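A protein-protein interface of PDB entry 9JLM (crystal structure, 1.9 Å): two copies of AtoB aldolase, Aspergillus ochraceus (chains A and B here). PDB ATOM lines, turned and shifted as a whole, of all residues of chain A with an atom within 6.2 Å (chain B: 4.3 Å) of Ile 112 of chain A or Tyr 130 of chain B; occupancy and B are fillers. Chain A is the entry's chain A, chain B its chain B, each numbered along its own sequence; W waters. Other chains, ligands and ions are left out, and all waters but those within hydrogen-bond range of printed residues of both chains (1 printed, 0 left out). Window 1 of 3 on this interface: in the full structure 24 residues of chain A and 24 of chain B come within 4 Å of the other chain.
O of Glu 110 of chain A is in hydrogen-bond range of OH of Tyr 130 of chain B. The side-chain hydroxyl of Tyr 130 of chain B sits at hydrogen-bond distance from the backbone NH of Asp 132 of chain A (3.2 Å).
Among the printed residues, pairs that only touch across the chains: His 95 of chain A with Leu 43 of chain B, Glu 110 of chain A with Leu 43 of chain B, Glu 110 of chain A with Pro 44 of chain B, Phe 111 of chain A with Tyr 130 of chain B, Ile 112 of chain A with Ile 114 of chain B, Ile 112 of chain A with Tyr 130 of chain B, Tyr 130 of chain A with Phe 111 of chain B, Tyr 130 of chain A with Ile 112 of chain B, Tyr 130 of chain A with Tyr 130 of chain B, Tyr 130 of chain A with Val 131 of chain B, Val 131 of chain A with Tyr 130 of chain B and Asp 132 of chain A with Pro 44 of chain B.
Of the printed residues of chain B, Ile 112 of chain A touches Ile 114 (3.9 Å) and Tyr 130 (3.6 Å). Of chain A, only Glu 110, Phe 111, Ile 112, Tyr 130, Val 131 and Asp 132 come within 4 Å of Tyr 130 of chain B. Of the printed residues of chain B, Phe 111 of chain A touches Tyr 130 (3.9 Å). Of the printed residues of chain A, Val 131 of chain B touches Tyr 130. Of the printed residues of chain A, Ile 114 of chain B touches Ile 112 (3.9 Å). Met 96 of chain A touches none of the printed residues of chain B. The nearest residue of chain A that does not touch Tyr 130 of chain B is His 95 of chain A (5.4 Å).
Phe 111 of chain A touches Tyr 130 of chain B, and with the chains exchanged Tyr 130 of chain A touches Phe 111 of chain B. Ile 112 of chain A touches Tyr 130 of chain B, and with the chains exchanged Tyr 130 of chain A touches Ile 112 of chain B. Tyr 130 of chain B touches its own counterpart, Tyr 130 of chain A. Tyr 130 of chain A touches Val 131 of chain B, and with the chains exchanged Val 131 of chain A touches Tyr 130 of chain B. Positions printed for both chains: 111, 112, 114, 129, 130 and 131. Of the 14 pairs that touch across the chains among the printed residues, 7 have their exchanged pair printed and touching as well.
The backbone carbonyl oxygen of Ile 112 of chain A sits at hydrogen-bond distance from the backbone NH of Tyr 130 of chain A. A ring nitrogen (NE2) of His 95 of chain A sits at hydrogen-bond distance from the side-chain carboxylate (OE2) of Glu 110 of chain A (2.6 Å). The backbone NH of Tyr 130 of chain B sits at hydrogen-bond distance from the backbone carbonyl oxygen of Ile 112 of chain B (2.8 Å). O of Leu 43 of chain B is in hydrogen-bond range of N of Val 131 of chain B, at 3.0 Å. O of Met 96 of chain A sits at hydrogen-bond distance from N of Phe 111 of chain A (2.9 Å). The backbone NH of Leu 43 of chain B sits at hydrogen-bond distance from the backbone carbonyl oxygen of Glu 129 of chain B, 2.6 Å away.
Water W1 lies within hydrogen-bond range of O of Val 131 of chain A (2.7 Å), O of Val 131 of chain B (2.8 Å) and N of Thr 133 of chain A (2.9 Å).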
ATOM      1  N   VAL A  93      26.137 -29.458  36.621  1.00  0.00           N
ATOM      2  CA  VAL A  93      25.380 -29.429  35.368  1.00  0.00           C
ATOM      3  C   VAL A  93      24.422 -30.615  35.350  1.00  0.00           C
ATOM      4  O   VAL A  93      24.838 -31.764  35.554  1.00  0.00           O
ATOM      5  CB  VAL A  93      26.292 -29.451  34.122  1.00  0.00           C
ATOM      6  CG1 VAL A  93      25.480 -29.199  32.865  1.00  0.00           C
ATOM      7  CG2 VAL A  93      27.402 -28.409  34.239  1.00  0.00           C
ATOM      8  N   PHE A  94      23.149 -30.334  35.126  1.00  0.00           N
ATOM      9  CA  PHE A  94      22.128 -31.345  34.910  1.00  0.00           C
ATOM     10  C   PHE A  94      21.606 -31.279  33.481  1.00  0.00           C
ATOM     11  O   PHE A  94      21.579 -30.212  32.860  1.00  0.00           O
ATOM     12  CB  PHE A  94      20.928 -31.156  35.846  1.00  0.00           C
ATOM     13  CG  PHE A  94      21.253 -31.229  37.316  1.00  0.00           C
ATOM     14  CD1 PHE A  94      21.708 -32.392  37.883  1.00  0.00           C
ATOM     15  CD2 PHE A  94      21.008 -30.142  38.146  1.00  0.00           C
ATOM     16  CE1 PHE A  94      21.975 -32.461  39.243  1.00  0.00           C
ATOM     17  CE2 PHE A  94      21.266 -30.203  39.505  1.00  0.00           C
ATOM     18  CZ  PHE A  94      21.748 -31.370  40.055  1.00  0.00           C
ATOM     19  N   HIS A  95      21.159 -32.438  32.984  1.00  0.00           N
ATOM     20  CA  HIS A  95      20.368 -32.569  31.761  1.00  0.00           C
ATOM     21  C   HIS A  95      18.955 -32.880  32.244  1.00  0.00           C
ATOM     22  O   HIS A  95      18.736 -33.937  32.838  1.00  0.00           O
ATOM     23  CB  HIS A  95      20.927 -33.695  30.875  1.00  0.00           C
ATOM     24  CG  HIS A  95      20.337 -33.757  29.495  1.00  0.00           C
ATOM     25  ND1 HIS A  95      20.551 -34.819  28.644  1.00  0.00           N
ATOM     26  CD2 HIS A  95      19.553 -32.887  28.817  1.00  0.00           C
ATOM     27  CE1 HIS A  95      19.916 -34.608  27.505  1.00  0.00           C
ATOM     28  NE2 HIS A  95      19.307 -33.440  27.580  1.00  0.00           N
ATOM     29  N   MET A  96      18.005 -31.958  32.026  1.00  0.00           N
ATOM     30  CA  MET A  96      16.731 -31.968  32.749  1.00  0.00           C
ATOM     31  C   MET A  96      15.546 -31.928  31.800  1.00  0.00           C
ATOM     32  O   MET A  96      15.637 -31.454  30.664  1.00  0.00           O
ATOM     33  CB  MET A  96      16.576 -30.766  33.708  1.00  0.00           C
ATOM     34  CG  MET A  96      17.574 -30.692  34.847  1.00  0.00           C
ATOM     35  SD  MET A  96      17.407 -32.046  36.019  1.00  0.00           S
ATOM     36  CE  MET A  96      15.808 -31.726  36.759  1.00  0.00           C
ATOM     37  N   ASN A 109       9.452 -29.300  28.393  1.00  0.00           N
ATOM     38  CA  ASN A 109      10.622 -29.150  27.539  1.00  0.00           C
ATOM     39  C   ASN A 109      11.847 -29.752  28.210  1.00  0.00           C
ATOM     40  O   ASN A 109      11.803 -30.207  29.357  1.00  0.00           O
ATOM     41  CB  ASN A 109      10.892 -27.691  27.195  1.00  0.00           C
ATOM     42  CG  ASN A 109       9.932 -27.164  26.195  1.00  0.00           C
ATOM     43  OD1 ASN A 109       9.827 -27.701  25.090  1.00  0.00           O
ATOM     44  ND2 ASN A 109       9.192 -26.117  26.573  1.00  0.00           N
ATOM     45  N   GLU A 110      12.946 -29.733  27.463  1.00  0.00           N
ATOM     46  CA  GLU A 110      14.238 -30.274  27.857  1.00  0.00           C
ATOM     47  C   GLU A 110      15.236 -29.125  27.964  1.00  0.00           C
ATOM     48  O   GLU A 110      15.205 -28.187  27.150  1.00  0.00           O
ATOM     49  CB  GLU A 110      14.700 -31.313  26.824  1.00  0.00           C
ATOM     50  CG  GLU A 110      16.139 -31.792  26.915  1.00  0.00           C
ATOM     51  CD  GLU A 110      16.479 -32.735  25.764  1.00  0.00           C
ATOM     52  OE1 GLU A 110      15.540 -33.152  25.063  1.00  0.00           O
ATOM     53  OE2 GLU A 110      17.667 -33.048  25.545  1.00  0.00           O
ATOM     54  N   PHE A 111      16.124 -29.205  28.967  1.00  0.00           N
ATOM     55  CA  PHE A 111      17.019 -28.113  29.328  1.00  0.00           C
ATOM     56  C   PHE A 111      18.394 -28.639  29.719  1.00  0.00           C
ATOM     57  O   PHE A 111      18.539 -29.776  30.179  1.00  0.00           O
ATOM     58  CB  PHE A 111      16.538 -27.312  30.554  1.00  0.00           C
ATOM     59  CG  PHE A 111      15.120 -26.788  30.479  1.00  0.00           C
ATOM     60  CD1 PHE A 111      14.034 -27.640  30.604  1.00  0.00           C
ATOM     61  CD2 PHE A 111      14.894 -25.414  30.420  1.00  0.00           C
ATOM     62  CE1 PHE A 111      12.727 -27.131  30.581  1.00  0.00           C
ATOM     63  CE2 PHE A 111      13.611 -24.899  30.409  1.00  0.00           C
ATOM     64  CZ  PHE A 111      12.526 -25.746  30.491  1.00  0.00           C
ATOM     65  N   ILE A 112      19.389 -27.755  29.605  1.00  0.00           N
ATOM     66  CA  ILE A 112      20.626 -27.830  30.380  1.00  0.00           C
ATOM     67  C   ILE A 112      20.531 -26.808  31.513  1.00  0.00           C
ATOM     68  O   ILE A 112      20.212 -25.635  31.281  1.00  0.00           O
ATOM     69  CB  ILE A 112      21.876 -27.556  29.521  1.00  0.00           C
ATOM     70  CG1 ILE A 112      22.024 -28.568  28.383  1.00  0.00           C
ATOM     71  CG2 ILE A 112      23.130 -27.558  30.404  1.00  0.00           C
ATOM     72  CD1 ILE A 112      22.398 -29.940  28.819  1.00  0.00           C
ATOM     73  N   PHE A 113      20.779 -27.254  32.734  1.00  0.00           N
ATOM     74  CA  PHE A 113      20.919 -26.379  33.886  1.00  0.00           C
ATOM     75  C   PHE A 113      22.370 -26.389  34.353  1.00  0.00           C
ATOM     76  O   PHE A 113      23.018 -27.441  34.342  1.00  0.00           O
ATOM     77  CB  PHE A 113      19.991 -26.832  35.022  1.00  0.00           C
ATOM     78  CG  PHE A 113      18.580 -26.334  34.887  1.00  0.00           C
ATOM     79  CD1 PHE A 113      17.645 -27.035  34.125  1.00  0.00           C
ATOM     80  CD2 PHE A 113      18.194 -25.154  35.516  1.00  0.00           C
ATOM     81  CE1 PHE A 113      16.355 -26.574  33.996  1.00  0.00           C
ATOM     82  CE2 PHE A 113      16.898 -24.674  35.395  1.00  0.00           C
ATOM     83  CZ  PHE A 113      15.970 -25.387  34.624  1.00  0.00           C
ATOM     84  N   ILE A 114      22.871 -25.218  34.762  1.00  0.00           N
ATOM     85  CA  ILE A 114      24.217 -25.054  35.318  1.00  0.00           C
ATOM     86  C   ILE A 114      24.100 -24.271  36.623  1.00  0.00           C
ATOM     87  O   ILE A 114      23.767 -23.078  36.613  1.00  0.00           O
ATOM     88  CB  ILE A 114      25.175 -24.339  34.347  1.00  0.00           C
ATOM     89  CG1 ILE A 114      25.269 -25.093  33.022  1.00  0.00           C
ATOM     90  CG2 ILE A 114      26.576 -24.185  34.982  1.00  0.00           C
ATOM     91  CD1 ILE A 114      25.961 -24.303  31.937  1.00  0.00           C
ATOM     92  N   ALA A 128      21.734 -21.014  35.783  1.00  0.00           N
ATOM     93  CA  ALA A 128      21.686 -20.781  34.349  1.00  0.00           C
ATOM     94  C   ALA A 128      20.946 -21.938  33.693  1.00  0.00           C
ATOM     95  O   ALA A 128      21.216 -23.101  34.003  1.00  0.00           O
ATOM     96  CB  ALA A 128      23.103 -20.637  33.769  1.00  0.00           C
ATOM     97  N   GLU A 129      19.997 -21.628  32.810  1.00  0.00           N
ATOM     98  CA  GLU A 129      19.282 -22.660  32.068  1.00  0.00           C
ATOM     99  C   GLU A 129      19.340 -22.339  30.587  1.00  0.00           C
ATOM    100  O   GLU A 129      19.007 -21.225  30.176  1.00  0.00           O
ATOM    101  CB  GLU A 129      17.820 -22.802  32.508  1.00  0.00           C
ATOM    102  CG  GLU A 129      16.970 -21.524  32.397  1.00  0.00           C
ATOM    103  CD  GLU A 129      15.575 -21.702  32.988  1.00  0.00           C
ATOM    104  OE1 GLU A 129      14.834 -22.600  32.546  1.00  0.00           O
ATOM    105  OE2 GLU A 129      15.224 -20.960  33.914  1.00  0.00           O
ATOM    106  N   TYR A 130      19.761 -23.316  29.793  1.00  0.00           N
ATOM    107  CA  TYR A 130      19.699 -23.220  28.343  1.00  0.00           C
ATOM    108  C   TYR A 130      18.413 -23.898  27.917  1.00  0.00           C
ATOM    109  O   TYR A 130      18.136 -25.030  28.317  1.00  0.00           O
ATOM    110  CB  TYR A 130      20.904 -23.863  27.660  1.00  0.00           C
ATOM    111  CG  TYR A 130      21.108 -23.410  26.227  1.00  0.00           C
ATOM    112  CD1 TYR A 130      20.119 -23.620  25.267  1.00  0.00           C
ATOM    113  CD2 TYR A 130      22.279 -22.774  25.832  1.00  0.00           C
ATOM    114  CE1 TYR A 130      20.290 -23.215  23.949  1.00  0.00           C
ATOM    115  CE2 TYR A 130      22.469 -22.377  24.511  1.00  0.00           C
ATOM    116  CZ  TYR A 130      21.456 -22.600  23.574  1.00  0.00           C
ATOM    117  OH  TYR A 130      21.597 -22.212  22.261  1.00  0.00           O
ATOM    118  N   VAL A 131      17.650 -23.190  27.099  1.00  0.00           N
ATOM    119  CA  VAL A 131      16.233 -23.395  26.896  1.00  0.00           C
ATOM    120  C   VAL A 131      16.013 -23.805  25.440  1.00  0.00           C
ATOM    121  O   VAL A 131      16.863 -23.587  24.575  1.00  0.00           O
ATOM    122  CB  VAL A 131      15.502 -22.087  27.288  1.00  0.00           C
ATOM    123  CG1 VAL A 131      14.786 -21.433  26.142  1.00  0.00           C
ATOM    124  CG2 VAL A 131      14.672 -22.274  28.541  1.00  0.00           C
ATOM    125  N   ASP A 132      14.875 -24.446  25.186  1.00  0.00           N
ATOM    126  CA  ASP A 132      14.452 -24.831  23.833  1.00  0.00           C
ATOM    127  C   ASP A 132      13.795 -23.612  23.179  1.00  0.00           C
ATOM    128  O   ASP A 132      12.598 -23.382  23.316  1.00  0.00           O
ATOM    129  CB  ASP A 132      13.507 -26.027  23.924  1.00  0.00           C
ATOM    130  CG  ASP A 132      13.056 -26.542  22.584  1.00  0.00           C
ATOM    131  OD1 ASP A 132      13.199 -25.818  21.585  1.00  0.00           O
ATOM    132  OD2 ASP A 132      12.515 -27.676  22.543  1.00  0.00           O
ATOM    133  N   THR A 133      14.573 -22.826  22.430  1.00  0.00           N
ATOM    134  CA  THR A 133      14.078 -21.516  22.001  1.00  0.00           C
ATOM    135  C   THR A 133      12.875 -21.617  21.057  1.00  0.00           C
ATOM    136  O   THR A 133      11.949 -20.797  21.139  1.00  0.00           O
ATOM    137  CB  THR A 133      15.200 -20.715  21.357  1.00  0.00           C
ATOM    138  OG1 THR A 133      15.711 -21.426  20.223  1.00  0.00           O
ATOM    139  CG2 THR A 133      16.313 -20.502  22.367  1.00  0.00           C
ATOM    140  N   LEU B  43      21.287 -31.837  21.137  1.00  0.00           N
ATOM    141  CA  LEU B  43      20.112 -31.632  21.977  1.00  0.00           C
ATOM    142  C   LEU B  43      19.448 -30.312  21.612  1.00  0.00           C
ATOM    143  O   LEU B  43      20.110 -29.415  21.083  1.00  0.00           O
ATOM    144  CB  LEU B  43      20.472 -31.609  23.465  1.00  0.00           C
ATOM    145  CG  LEU B  43      21.668 -32.397  23.994  1.00  0.00           C
ATOM    146  CD1 LEU B  43      21.798 -32.152  25.492  1.00  0.00           C
ATOM    147  CD2 LEU B  43      21.604 -33.892  23.689  1.00  0.00           C
ATOM    148  N   PRO B  44      18.138 -30.135  21.885  1.00  0.00           N
ATOM    149  CA  PRO B  44      17.205 -31.078  22.505  1.00  0.00           C
ATOM    150  C   PRO B  44      16.697 -32.130  21.527  1.00  0.00           C
ATOM    151  O   PRO B  44      16.779 -31.911  20.326  1.00  0.00           O
ATOM    152  CB  PRO B  44      16.051 -30.169  22.970  1.00  0.00           C
ATOM    153  CG  PRO B  44      16.064 -29.068  22.029  1.00  0.00           C
ATOM    154  CD  PRO B  44      17.524 -28.807  21.724  1.00  0.00           C
ATOM    155  N   PHE B 111      25.874 -22.009  22.185  1.00  0.00           N
ATOM    156  CA  PHE B 111      25.683 -23.435  22.456  1.00  0.00           C
ATOM    157  C   PHE B 111      26.149 -23.770  23.863  1.00  0.00           C
ATOM    158  O   PHE B 111      26.978 -23.068  24.448  1.00  0.00           O
ATOM    159  CB  PHE B 111      26.504 -24.346  21.526  1.00  0.00           C
ATOM    160  CG  PHE B 111      26.304 -24.105  20.060  1.00  0.00           C
ATOM    161  CD1 PHE B 111      26.840 -22.985  19.440  1.00  0.00           C
ATOM    162  CD2 PHE B 111      25.643 -25.055  19.279  1.00  0.00           C
ATOM    163  CE1 PHE B 111      26.671 -22.785  18.065  1.00  0.00           C
ATOM    164  CE2 PHE B 111      25.474 -24.871  17.913  1.00  0.00           C
ATOM    165  CZ  PHE B 111      25.984 -23.740  17.306  1.00  0.00           C
ATOM    166  N   ILE B 112      25.661 -24.898  24.375  1.00  0.00           N
ATOM    167  CA  ILE B 112      26.361 -25.660  25.408  1.00  0.00           C
ATOM    168  C   ILE B 112      26.949 -26.898  24.741  1.00  0.00           C
ATOM    169  O   ILE B 112      26.264 -27.567  23.963  1.00  0.00           O
ATOM    170  CB  ILE B 112      25.446 -26.072  26.574  1.00  0.00           C
ATOM    171  CG1 ILE B 112      24.745 -24.862  27.198  1.00  0.00           C
ATOM    172  CG2 ILE B 112      26.270 -26.831  27.629  1.00  0.00           C
ATOM    173  CD1 ILE B 112      25.657 -23.871  27.834  1.00  0.00           C
ATOM    174  N   ILE B 114      29.019 -30.565  25.703  1.00  0.00           N
ATOM    175  CA  ILE B 114      29.353 -31.482  26.795  1.00  0.00           C
ATOM    176  C   ILE B 114      30.203 -32.601  26.209  1.00  0.00           C
ATOM    177  O   ILE B 114      29.728 -33.367  25.365  1.00  0.00           O
ATOM    178  CB  ILE B 114      28.113 -32.050  27.491  1.00  0.00           C
ATOM    179  CG1 ILE B 114      27.251 -30.922  28.044  1.00  0.00           C
ATOM    180  CG2 ILE B 114      28.530 -33.052  28.603  1.00  0.00           C
ATOM    181  CD1 ILE B 114      26.055 -31.401  28.816  1.00  0.00           C
ATOM    182  N   GLU B 129      25.858 -31.364  22.053  1.00  0.00           N
ATOM    183  CA  GLU B 129      25.672 -29.924  21.960  1.00  0.00           C
ATOM    184  C   GLU B 129      24.191 -29.613  22.084  1.00  0.00           C
ATOM    185  O   GLU B 129      23.361 -30.273  21.451  1.00  0.00           O
ATOM    186  CB  GLU B 129      26.231 -29.359  20.650  1.00  0.00           C
ATOM    187  CG  GLU B 129      25.780 -30.068  19.403  1.00  0.00           C
ATOM    188  CD  GLU B 129      26.327 -29.402  18.146  1.00  0.00           C
ATOM    189  OE1 GLU B 129      25.823 -28.322  17.757  1.00  0.00           O
ATOM    190  OE2 GLU B 129      27.288 -29.935  17.566  1.00  0.00           O
ATOM    191  N   TYR B 130      23.864 -28.629  22.914  1.00  0.00           N
ATOM    192  CA  TYR B 130      22.516 -28.071  22.982  1.00  0.00           C
ATOM    193  C   TYR B 130      22.496 -26.823  22.104  1.00  0.00           C
ATOM    194  O   TYR B 130      23.273 -25.888  22.331  1.00  0.00           O
ATOM    195  CB  TYR B 130      22.118 -27.750  24.424  1.00  0.00           C
ATOM    196  CG  TYR B 130      20.619 -27.624  24.646  1.00  0.00           C
ATOM    197  CD1 TYR B 130      19.895 -26.644  23.986  1.00  0.00           C
ATOM    198  CD2 TYR B 130      19.931 -28.491  25.496  1.00  0.00           C
ATOM    199  CE1 TYR B 130      18.530 -26.502  24.173  1.00  0.00           C
ATOM    200  CE2 TYR B 130      18.541 -28.356  25.701  1.00  0.00           C
ATOM    201  CZ  TYR B 130      17.853 -27.349  25.023  1.00  0.00           C
ATOM    202  OH  TYR B 130      16.486 -27.164  25.159  1.00  0.00           O
ATOM    203  N   VAL B 131      21.627 -26.814  21.095  1.00  0.00           N
ATOM    204  CA  VAL B 131      21.651 -25.794  20.060  1.00  0.00           C
ATOM    205  C   VAL B 131      20.484 -24.828  20.255  1.00  0.00           C
ATOM    206  O   VAL B 131      19.588 -25.048  21.069  1.00  0.00           O
ATOM    207  CB  VAL B 131      21.611 -26.403  18.645  1.00  0.00           C
ATOM    208  CG1 VAL B 131      22.697 -27.464  18.478  1.00  0.00           C
ATOM    209  CG2 VAL B 131      20.229 -26.970  18.370  1.00  0.00           C
HETATM  210  O   HOH W   1      17.210 -23.933  21.906  1.00  0.00           O
